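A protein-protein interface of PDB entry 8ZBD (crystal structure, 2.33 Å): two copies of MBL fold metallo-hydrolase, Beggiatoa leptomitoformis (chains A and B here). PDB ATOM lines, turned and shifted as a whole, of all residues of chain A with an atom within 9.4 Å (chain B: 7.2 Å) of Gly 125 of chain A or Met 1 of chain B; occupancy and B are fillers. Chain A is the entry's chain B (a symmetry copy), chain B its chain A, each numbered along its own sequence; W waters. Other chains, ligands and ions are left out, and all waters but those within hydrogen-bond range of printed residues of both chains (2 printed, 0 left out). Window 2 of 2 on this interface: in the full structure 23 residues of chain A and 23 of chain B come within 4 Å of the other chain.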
ATOM      1  N   MET A   1      14.762  -8.305 -28.668  1.00  0.00           N
ATOM      2  CA  MET A   1      14.598  -9.171 -29.837  1.00  0.00           C
ATOM      3  C   MET A   1      13.749  -8.482 -30.888  1.00  0.00           C
ATOM      4  O   MET A   1      12.756  -7.855 -30.553  1.00  0.00           O
ATOM      5  CB  MET A   1      13.967 -10.497 -29.414  1.00  0.00           C
ATOM      6  CG  MET A   1      13.291 -11.202 -30.539  1.00  0.00           C
ATOM      7  SD  MET A   1      12.519 -12.728 -30.033  1.00  0.00           S
ATOM      8  CE  MET A   1      10.900 -12.376 -30.698  1.00  0.00           C
ATOM      9  N   VAL A 122       8.636 -18.485 -27.009  1.00  0.00           N
ATOM     10  CA  VAL A 122       9.860 -17.738 -26.746  1.00  0.00           C
ATOM     11  C   VAL A 122       9.658 -16.920 -25.473  1.00  0.00           C
ATOM     12  O   VAL A 122       8.628 -16.249 -25.314  1.00  0.00           O
ATOM     13  CB  VAL A 122      10.220 -16.805 -27.922  1.00  0.00           C
ATOM     14  CG1 VAL A 122      11.366 -15.868 -27.546  1.00  0.00           C
ATOM     15  CG2 VAL A 122      10.569 -17.610 -29.150  1.00  0.00           C
ATOM     16  N   ASP A 123      10.645 -16.968 -24.577  1.00  0.00           N
ATOM     17  CA  ASP A 123      10.673 -16.133 -23.381  1.00  0.00           C
ATOM     18  C   ASP A 123      11.438 -14.846 -23.687  1.00  0.00           C
ATOM     19  O   ASP A 123      12.603 -14.900 -24.079  1.00  0.00           O
ATOM     20  CB  ASP A 123      11.336 -16.901 -22.244  1.00  0.00           C
ATOM     21  CG  ASP A 123      11.252 -16.189 -20.910  1.00  0.00           C
ATOM     22  OD1 ASP A 123      10.817 -15.008 -20.831  1.00  0.00           O
ATOM     23  OD2 ASP A 123      11.633 -16.845 -19.916  1.00  0.00           O
ATOM     24  N   THR A 124      10.783 -13.694 -23.533  1.00  0.00           N
ATOM     25  CA  THR A 124      11.427 -12.409 -23.784  1.00  0.00           C
ATOM     26  C   THR A 124      12.054 -11.811 -22.538  1.00  0.00           C
ATOM     27  O   THR A 124      12.679 -10.755 -22.626  1.00  0.00           O
ATOM     28  CB  THR A 124      10.426 -11.394 -24.345  1.00  0.00           C
ATOM     29  OG1 THR A 124       9.609 -10.894 -23.278  1.00  0.00           O
ATOM     30  CG2 THR A 124       9.549 -12.016 -25.414  1.00  0.00           C
ATOM     31  N   GLY A 125      11.896 -12.451 -21.383  1.00  0.00           N
ATOM     32  CA  GLY A 125      12.295 -11.919 -20.118  1.00  0.00           C
ATOM     33  C   GLY A 125      11.142 -11.309 -19.352  1.00  0.00           C
ATOM     34  O   GLY A 125      11.159 -11.309 -18.119  1.00  0.00           O
ATOM     35  N   THR A 126      10.127 -10.825 -20.064  1.00  0.00           N
ATOM     36  CA  THR A 126       8.911 -10.274 -19.485  1.00  0.00           C
ATOM     37  C   THR A 126       7.672 -11.057 -19.886  1.00  0.00           C
ATOM     38  O   THR A 126       6.798 -11.287 -19.046  1.00  0.00           O
ATOM     39  CB  THR A 126       8.756  -8.794 -19.910  1.00  0.00           C
ATOM     40  OG1 THR A 126       9.828  -8.033 -19.363  1.00  0.00           O
ATOM     41  CG2 THR A 126       7.435  -8.202 -19.415  1.00  0.00           C
ATOM     42  N   HIS A 127       7.574 -11.462 -21.151  1.00  0.00           N
ATOM     43  CA  HIS A 127       6.460 -12.233 -21.689  1.00  0.00           C
ATOM     44  C   HIS A 127       6.958 -13.558 -22.250  1.00  0.00           C
ATOM     45  O   HIS A 127       8.064 -13.635 -22.800  1.00  0.00           O
ATOM     46  CB  HIS A 127       5.752 -11.523 -22.844  1.00  0.00           C
ATOM     47  CG  HIS A 127       5.083 -10.243 -22.466  1.00  0.00           C
ATOM     48  ND1 HIS A 127       5.749  -9.033 -22.440  1.00  0.00           N
ATOM     49  CD2 HIS A 127       3.797  -9.975 -22.139  1.00  0.00           C
ATOM     50  CE1 HIS A 127       4.903  -8.078 -22.093  1.00  0.00           C
ATOM     51  NE2 HIS A 127       3.712  -8.621 -21.908  1.00  0.00           N
ATOM     52  N   LEU A 128       6.118 -14.594 -22.123  1.00  0.00           N
ATOM     53  CA  LEU A 128       6.165 -15.760 -23.003  1.00  0.00           C
ATOM     54  C   LEU A 128       5.347 -15.449 -24.248  1.00  0.00           C
ATOM     55  O   LEU A 128       4.183 -15.043 -24.137  1.00  0.00           O
ATOM     56  CB  LEU A 128       5.584 -17.000 -22.324  1.00  0.00           C
ATOM     57  CG  LEU A 128       6.435 -17.891 -21.429  1.00  0.00           C
ATOM     58  CD1 LEU A 128       5.753 -19.224 -21.319  1.00  0.00           C
ATOM     59  CD2 LEU A 128       7.855 -18.037 -21.951  1.00  0.00           C
ATOM     60  N   MET A 129       5.951 -15.614 -25.427  1.00  0.00           N
ATOM     61  CA  MET A 129       5.216 -15.486 -26.682  1.00  0.00           C
ATOM     62  C   MET A 129       4.891 -16.875 -27.204  1.00  0.00           C
ATOM     63  O   MET A 129       5.796 -17.681 -27.441  1.00  0.00           O
ATOM     64  CB  MET A 129       5.987 -14.703 -27.749  1.00  0.00           C
ATOM     65  CG  MET A 129       6.696 -13.444 -27.272  1.00  0.00           C
ATOM     66  SD  MET A 129       7.863 -12.874 -28.519  1.00  0.00           S
ATOM     67  CE  MET A 129       6.767 -12.035 -29.640  1.00  0.00           C
ATOM     68  N   GLU A 168      -0.452 -14.571 -18.515  1.00  0.00           N
ATOM     69  CA  GLU A 168      -0.008 -13.462 -19.341  1.00  0.00           C
ATOM     70  C   GLU A 168       0.647 -13.899 -20.638  1.00  0.00           C
ATOM     71  O   GLU A 168       1.063 -13.030 -21.415  1.00  0.00           O
ATOM     72  CB  GLU A 168       0.961 -12.590 -18.543  1.00  0.00           C
ATOM     73  CG  GLU A 168       0.257 -11.753 -17.468  1.00  0.00           C
ATOM     74  CD  GLU A 168      -0.233 -12.571 -16.264  1.00  0.00           C
ATOM     75  OE1 GLU A 168       0.300 -13.701 -15.989  1.00  0.00           O
ATOM     76  OE2 GLU A 168      -1.178 -12.080 -15.603  1.00  0.00           O
ATOM     77  N   MET B   1      11.326  -8.567 -16.456  1.00  0.00           N
ATOM     78  CA  MET B   1      10.407  -7.812 -15.614  1.00  0.00           C
ATOM     79  C   MET B   1       9.253  -8.704 -15.140  1.00  0.00           C
ATOM     80  O   MET B   1       8.690  -9.460 -15.921  1.00  0.00           O
ATOM     81  CB  MET B   1       9.867  -6.626 -16.387  1.00  0.00           C
ATOM     82  CG  MET B   1       8.927  -5.762 -15.623  1.00  0.00           C
ATOM     83  SD  MET B   1       8.350  -4.383 -16.644  1.00  0.00           S
ATOM     84  CE  MET B   1       6.790  -5.046 -17.243  1.00  0.00           C
ATOM     85  N   ILE B   2       8.918  -8.626 -13.865  1.00  0.00           N
ATOM     86  CA  ILE B   2       7.754  -9.325 -13.342  1.00  0.00           C
ATOM     87  C   ILE B   2       6.504  -8.572 -13.767  1.00  0.00           C
ATOM     88  O   ILE B   2       6.381  -7.368 -13.530  1.00  0.00           O
ATOM     89  CB  ILE B   2       7.834  -9.441 -11.815  1.00  0.00           C
ATOM     90  CG1 ILE B   2       9.090 -10.223 -11.420  1.00  0.00           C
ATOM     91  CG2 ILE B   2       6.558 -10.069 -11.245  1.00  0.00           C
ATOM     92  CD1 ILE B   2       9.629  -9.840 -10.044  1.00  0.00           C
ATOM     93  N   PHE B   3       5.575  -9.273 -14.395  1.00  0.00           N
ATOM     94  CA  PHE B   3       4.377  -8.649 -14.922  1.00  0.00           C
ATOM     95  C   PHE B   3       3.151  -9.488 -14.594  1.00  0.00           C
ATOM     96  O   PHE B   3       3.122 -10.685 -14.893  1.00  0.00           O
ATOM     97  CB  PHE B   3       4.481  -8.457 -16.438  1.00  0.00           C
ATOM     98  CG  PHE B   3       3.228  -7.912 -17.039  1.00  0.00           C
ATOM     99  CD1 PHE B   3       2.718  -6.708 -16.601  1.00  0.00           C
ATOM    100  CD2 PHE B   3       2.525  -8.626 -18.000  1.00  0.00           C
ATOM    101  CE1 PHE B   3       1.548  -6.194 -17.136  1.00  0.00           C
ATOM    102  CE2 PHE B   3       1.348  -8.130 -18.528  1.00  0.00           C
ATOM    103  CZ  PHE B   3       0.852  -6.916 -18.092  1.00  0.00           C
ATOM    104  N   GLN B   4       2.118  -8.860 -14.026  1.00  0.00           N
ATOM    105  CA  GLN B   4       0.842  -9.537 -13.830  1.00  0.00           C
ATOM    106  C   GLN B   4      -0.302  -8.592 -14.153  1.00  0.00           C
ATOM    107  O   GLN B   4      -0.255  -7.399 -13.823  1.00  0.00           O
ATOM    108  CB  GLN B   4       0.689 -10.065 -12.405  1.00  0.00           C
ATOM    109  CG  GLN B   4       1.467 -11.350 -12.147  1.00  0.00           C
ATOM    110  CD  GLN B   4       1.033 -12.054 -10.882  1.00  0.00           C
ATOM    111  OE1 GLN B   4      -0.161 -12.165 -10.583  1.00  0.00           O
ATOM    112  NE2 GLN B   4       2.003 -12.526 -10.120  1.00  0.00           N
ATOM    113  N   LEU B  17       0.538  -5.102 -12.262  1.00  0.00           N
ATOM    114  CA  LEU B  17       1.680  -5.193 -11.368  1.00  0.00           C
ATOM    115  C   LEU B  17       2.938  -5.311 -12.217  1.00  0.00           C
ATOM    116  O   LEU B  17       3.049  -6.222 -13.042  1.00  0.00           O
ATOM    117  CB  LEU B  17       1.536  -6.394 -10.436  1.00  0.00           C
ATOM    118  CG  LEU B  17       2.657  -6.814  -9.476  1.00  0.00           C
ATOM    119  CD1 LEU B  17       2.081  -7.687  -8.371  1.00  0.00           C
ATOM    120  CD2 LEU B  17       3.736  -7.580 -10.181  1.00  0.00           C
ATOM    121  N   LEU B  18       3.881  -4.402 -12.007  1.00  0.00           N
ATOM    122  CA  LEU B  18       5.172  -4.429 -12.677  1.00  0.00           C
ATOM    123  C   LEU B  18       6.237  -4.464 -11.597  1.00  0.00           C
ATOM    124  O   LEU B  18       6.188  -3.662 -10.659  1.00  0.00           O
ATOM    125  CB  LEU B  18       5.370  -3.204 -13.580  1.00  0.00           C
ATOM    126  CG  LEU B  18       4.587  -3.065 -14.887  1.00  0.00           C
ATOM    127  CD1 LEU B  18       3.129  -2.764 -14.613  1.00  0.00           C
ATOM    128  CD2 LEU B  18       5.193  -1.965 -15.780  1.00  0.00           C
ATOM    129  N   GLY B  19       7.180  -5.389 -11.716  1.00  0.00           N
ATOM    130  CA  GLY B  19       8.211  -5.550 -10.710  1.00  0.00           C
ATOM    131  C   GLY B  19       9.595  -5.647 -11.317  1.00  0.00           C
ATOM    132  O   GLY B  19       9.785  -6.178 -12.411  1.00  0.00           O
ATOM    133  N   CYS B  20      10.572  -5.118 -10.581  1.00  0.00           N
ATOM    134  CA  CYS B  20      11.969  -5.221 -10.975  1.00  0.00           C
ATOM    135  C   CYS B  20      12.589  -6.412 -10.265  1.00  0.00           C
ATOM    136  O   CYS B  20      12.638  -6.420  -9.024  1.00  0.00           O
ATOM    137  CB  CYS B  20      12.734  -3.946 -10.634  1.00  0.00           C
ATOM    138  SG  CYS B  20      14.527  -4.088 -10.888  1.00  0.00           S
ATOM    139  N   PRO B  21      13.048  -7.438 -10.985  1.00  0.00           N
ATOM    140  CA  PRO B  21      13.587  -8.626 -10.293  1.00  0.00           C
ATOM    141  C   PRO B  21      14.897  -8.361  -9.559  1.00  0.00           C
ATOM    142  O   PRO B  21      15.236  -9.115  -8.642  1.00  0.00           O
ATOM    143  CB  PRO B  21      13.761  -9.644 -11.430  1.00  0.00           C
ATOM    144  CG  PRO B  21      13.998  -8.786 -12.656  1.00  0.00           C
ATOM    145  CD  PRO B  21      13.146  -7.548 -12.455  1.00  0.00           C
ATOM    146  N   VAL B 103      13.144  -0.637 -14.288  1.00  0.00           N
ATOM    147  CA  VAL B 103      11.988  -0.509 -15.161  1.00  0.00           C
ATOM    148  C   VAL B 103      11.636   0.970 -15.286  1.00  0.00           C
ATOM    149  O   VAL B 103      11.549   1.689 -14.283  1.00  0.00           O
ATOM    150  CB  VAL B 103      10.807  -1.331 -14.630  1.00  0.00           C
ATOM    151  CG1 VAL B 103       9.538  -0.971 -15.366  1.00  0.00           C
ATOM    152  CG2 VAL B 103      11.099  -2.800 -14.797  1.00  0.00           C
ATOM    153  N   GLN B 104      11.462   1.424 -16.520  1.00  0.00           N
ATOM    154  CA  GLN B 104      11.194   2.816 -16.851  1.00  0.00           C
ATOM    155  C   GLN B 104       9.771   2.924 -17.397  1.00  0.00           C
ATOM    156  O   GLN B 104       9.468   2.344 -18.449  1.00  0.00           O
ATOM    157  CB  GLN B 104      12.189   3.301 -17.901  1.00  0.00           C
ATOM    158  CG  GLN B 104      13.468   3.884 -17.380  1.00  0.00           C
ATOM    159  CD  GLN B 104      14.006   4.932 -18.337  1.00  0.00           C
ATOM    160  OE1 GLN B 104      13.763   6.122 -18.160  1.00  0.00           O
ATOM    161  NE2 GLN B 104      14.717   4.490 -19.377  1.00  0.00           N
ATOM    162  N   ILE B 105       8.919   3.693 -16.719  1.00  0.00           N
ATOM    163  CA  ILE B 105       7.531   3.871 -17.133  1.00  0.00           C
ATOM    164  C   ILE B 105       7.368   5.261 -17.741  1.00  0.00           C
ATOM    165  O   ILE B 105       7.637   6.270 -17.079  1.00  0.00           O
ATOM    166  CB  ILE B 105       6.569   3.669 -15.955  1.00  0.00           C
ATOM    167  CG1 ILE B 105       6.841   2.329 -15.271  1.00  0.00           C
ATOM    168  CG2 ILE B 105       5.124   3.746 -16.430  1.00  0.00           C
ATOM    169  CD1 ILE B 105       5.854   2.032 -14.183  1.00  0.00           C
ATOM    170  N   VAL B 122       5.805   0.937 -21.438  1.00  0.00           N
ATOM    171  CA  VAL B 122       7.056   0.343 -20.988  1.00  0.00           C
ATOM    172  C   VAL B 122       7.660  -0.453 -22.131  1.00  0.00           C
ATOM    173  O   VAL B 122       6.943  -1.138 -22.871  1.00  0.00           O
ATOM    174  CB  VAL B 122       6.840  -0.557 -19.764  1.00  0.00           C
ATOM    175  CG1 VAL B 122       8.042  -1.424 -19.531  1.00  0.00           C
ATOM    176  CG2 VAL B 122       6.576   0.300 -18.562  1.00  0.00           C
ATOM    177  N   ASP B 123       8.979  -0.358 -22.278  1.00  0.00           N
ATOM    178  CA  ASP B 123       9.726  -1.116 -23.274  1.00  0.00           C
ATOM    179  C   ASP B 123      10.381  -2.326 -22.612  1.00  0.00           C
ATOM    180  O   ASP B 123      11.268  -2.165 -21.771  1.00  0.00           O
ATOM    181  CB  ASP B 123      10.775  -0.219 -23.925  1.00  0.00           C
ATOM    182  CG  ASP B 123      11.496  -0.893 -25.075  1.00  0.00           C
ATOM    183  OD1 ASP B 123      11.358  -2.129 -25.258  1.00  0.00           O
ATOM    184  OD2 ASP B 123      12.204  -0.176 -25.812  1.00  0.00           O
ATOM    185  N   THR B 124       9.966  -3.533 -23.013  1.00  0.00           N
ATOM    186  CA  THR B 124      10.513  -4.772 -22.456  1.00  0.00           C
ATOM    187  C   THR B 124      11.791  -5.243 -23.148  1.00  0.00           C
ATOM    188  O   THR B 124      12.425  -6.177 -22.657  1.00  0.00           O
ATOM    189  CB  THR B 124       9.489  -5.941 -22.533  1.00  0.00           C
ATOM    190  OG1 THR B 124       9.501  -6.509 -23.852  1.00  0.00           O
ATOM    191  CG2 THR B 124       8.083  -5.507 -22.195  1.00  0.00           C
ATOM    192  N   THR B 126      11.553  -6.374 -26.345  1.00  0.00           N
ATOM    193  CA  THR B 126      10.876  -6.987 -27.479  1.00  0.00           C
ATOM    194  C   THR B 126       9.539  -6.333 -27.775  1.00  0.00           C
ATOM    195  O   THR B 126       9.168  -6.178 -28.939  1.00  0.00           O
ATOM    196  CB  THR B 126      10.653  -8.489 -27.204  1.00  0.00           C
ATOM    197  OG1 THR B 126      11.904  -9.121 -26.920  1.00  0.00           O
ATOM    198  CG2 THR B 126      10.028  -9.153 -28.379  1.00  0.00           C
ATOM    199  N   MET B 129       4.780  -2.103 -24.214  1.00  0.00           N
ATOM    200  CA  MET B 129       3.541  -2.391 -23.508  1.00  0.00           C
ATOM    201  C   MET B 129       2.831  -1.060 -23.251  1.00  0.00           C
ATOM    202  O   MET B 129       3.358  -0.214 -22.520  1.00  0.00           O
ATOM    203  CB  MET B 129       3.807  -3.070 -22.165  1.00  0.00           C
ATOM    204  CG  MET B 129       4.835  -4.153 -22.136  1.00  0.00           C
ATOM    205  SD  MET B 129       5.013  -4.899 -20.471  1.00  0.00           S
ATOM    206  CE  MET B 129       3.389  -5.569 -20.174  1.00  0.00           C
ATOM    207  N   PHE B 131      -0.161   0.672 -21.427  1.00  0.00           N
ATOM    208  CA  PHE B 131      -1.261   0.719 -20.465  1.00  0.00           C
ATOM    209  C   PHE B 131      -2.115   1.926 -20.829  1.00  0.00           C
ATOM    210  O   PHE B 131      -1.758   3.071 -20.536  1.00  0.00           O
ATOM    211  CB  PHE B 131      -0.706   0.769 -19.043  1.00  0.00           C
ATOM    212  CG  PHE B 131       0.266  -0.341 -18.760  1.00  0.00           C
ATOM    213  CD1 PHE B 131      -0.191  -1.624 -18.491  1.00  0.00           C
ATOM    214  CD2 PHE B 131       1.627  -0.128 -18.854  1.00  0.00           C
ATOM    215  CE1 PHE B 131       0.689  -2.666 -18.256  1.00  0.00           C
ATOM    216  CE2 PHE B 131       2.530  -1.172 -18.629  1.00  0.00           C
ATOM    217  CZ  PHE B 131       2.052  -2.445 -18.329  1.00  0.00           C
HETATM  218  O   HOH W   1       7.982  -8.707 -23.873  1.00  0.00           O
HETATM  219  O   HOH W   2      11.928  -8.341 -21.130  1.00  0.00           O
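Among the printed residues, pairs that only touch across the chains: Thr 124 of chain A with Thr 126 of chain B (3.7 Å), Thr 126 of chain A with Thr 124 of chain B (3.8 Å), His 127 of chain A with Met 129 of chain B (3.5 Å), Glu 168 of chain A with Phe 3 of chain B (3.9 Å) and Glu 168 of chain A with Gln 4 of chain B (3.7 Å).
The side-chain hydroxyl (OG1) of Thr 124 of chain B is in hydrogen-bond range of the backbone NH (N) of Thr 126 of chain B (3.2 Å). The backbone carbonyl oxygen (O) of Gln 4 of chain B lies within hydrogen-bond range of the backbone NH (N) of Leu 17 of chain B. The side-chain carboxylate (OD1) of Asp 123 of chain A lies within hydrogen-bond range of the backbone NH (N) of Gly 125 of chain A (2.8 Å). The side-chain hydroxyl (OG1) of Thr 124 of chain A is in hydrogen-bond range of the backbone NH (N) of Thr 126 of chain A (3.3 Å). The backbone carbonyl oxygen of Val 122 of chain B sits at hydrogen-bond distance from the backbone NH of Met 129 of chain B (2.7 Å). The backbone NH (N) of His 127 of chain A sits at hydrogen-bond distance from the side-chain hydroxyl (OG1) of Thr 124 of chain A (3.0 Å).
Printed residues of chain B that touch a printed residue of chain A: Met 1, Phe 3, Gln 4, Thr 124, Thr 126 and Met 129. Hydrophobic or aromatic side chains of chain B that line the printed part of chain A: Met 1, Phe 3 and Met 129. Of the 10 printed residues of chain A, 6 touch a printed residue of chain B. Printed residues of chain A that touch a printed residue of chain B: Met 1, Thr 124, Gly 125, Thr 126, His 127 and Glu 168. Hydrophobic or aromatic side chains of chain A within 4 Å of the printed part of chain B: Met 1 and His 127.
Of the printed residues of chain A, Met 1 of chain B touches Gly 125 and Thr 126. No residue of chain A comes within 4 Å of Ile 2 of chain B. Of the printed residues of chain B, Met 1 of chain A touches Thr 126. Printed residues of chain A within 4 Å of Gln 4 of chain B: Glu 168 (3.7 Å). Printed residues of chain B within 4 Å of His 127 of chain A: Met 129 (3.5 Å). The nearest residue of chain B that does not touch Gly 125 of chain A is Ile 2 of chain B (5.5 Å).
Met 1 of chain A touches Thr 126 of chain B, and with the chains exchanged Thr 126 of chain A touches Met 1 of chain B. Thr 124 of chain A touches Thr 126 of chain B, and with the chains exchanged Thr 126 of chain A touches Thr 124 of chain B. Positions printed for both chains: 1, 122, 123, 124, 126 and 129. Of the 8 pairs that touch across the chains among the printed residues, 4 have their exchanged pair printed and touching as well.
Water W1 lies within hydrogen-bond range of OG1 of Thr 124 of chain B (2.7 Å), ND1 of His 127 of chain A (2.7 Å) and OG1 of Thr 124 of chain A (2.8 Å). Water W2 lies within hydrogen-bond range of O of Thr 124 of chain B (2.7 Å), OG1 of Thr 126 of chain A (2.8 Å) and O of Thr 124 of chain A (2.9 Å).
The backbone carbonyl oxygen of Gly 125 of chain A lies within hydrogen-bond range of the backbone NH of Met 1 of chain B. N of Met 1 of chain A lies within hydrogen-bond range of OG1 of Thr 126 of chain B (3.4 Å). The backbone NH (N) of Met 1 of chain B lies close to the side-chain hydroxyl (OG1) of Thr 126 of chain A (3.3 Å).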
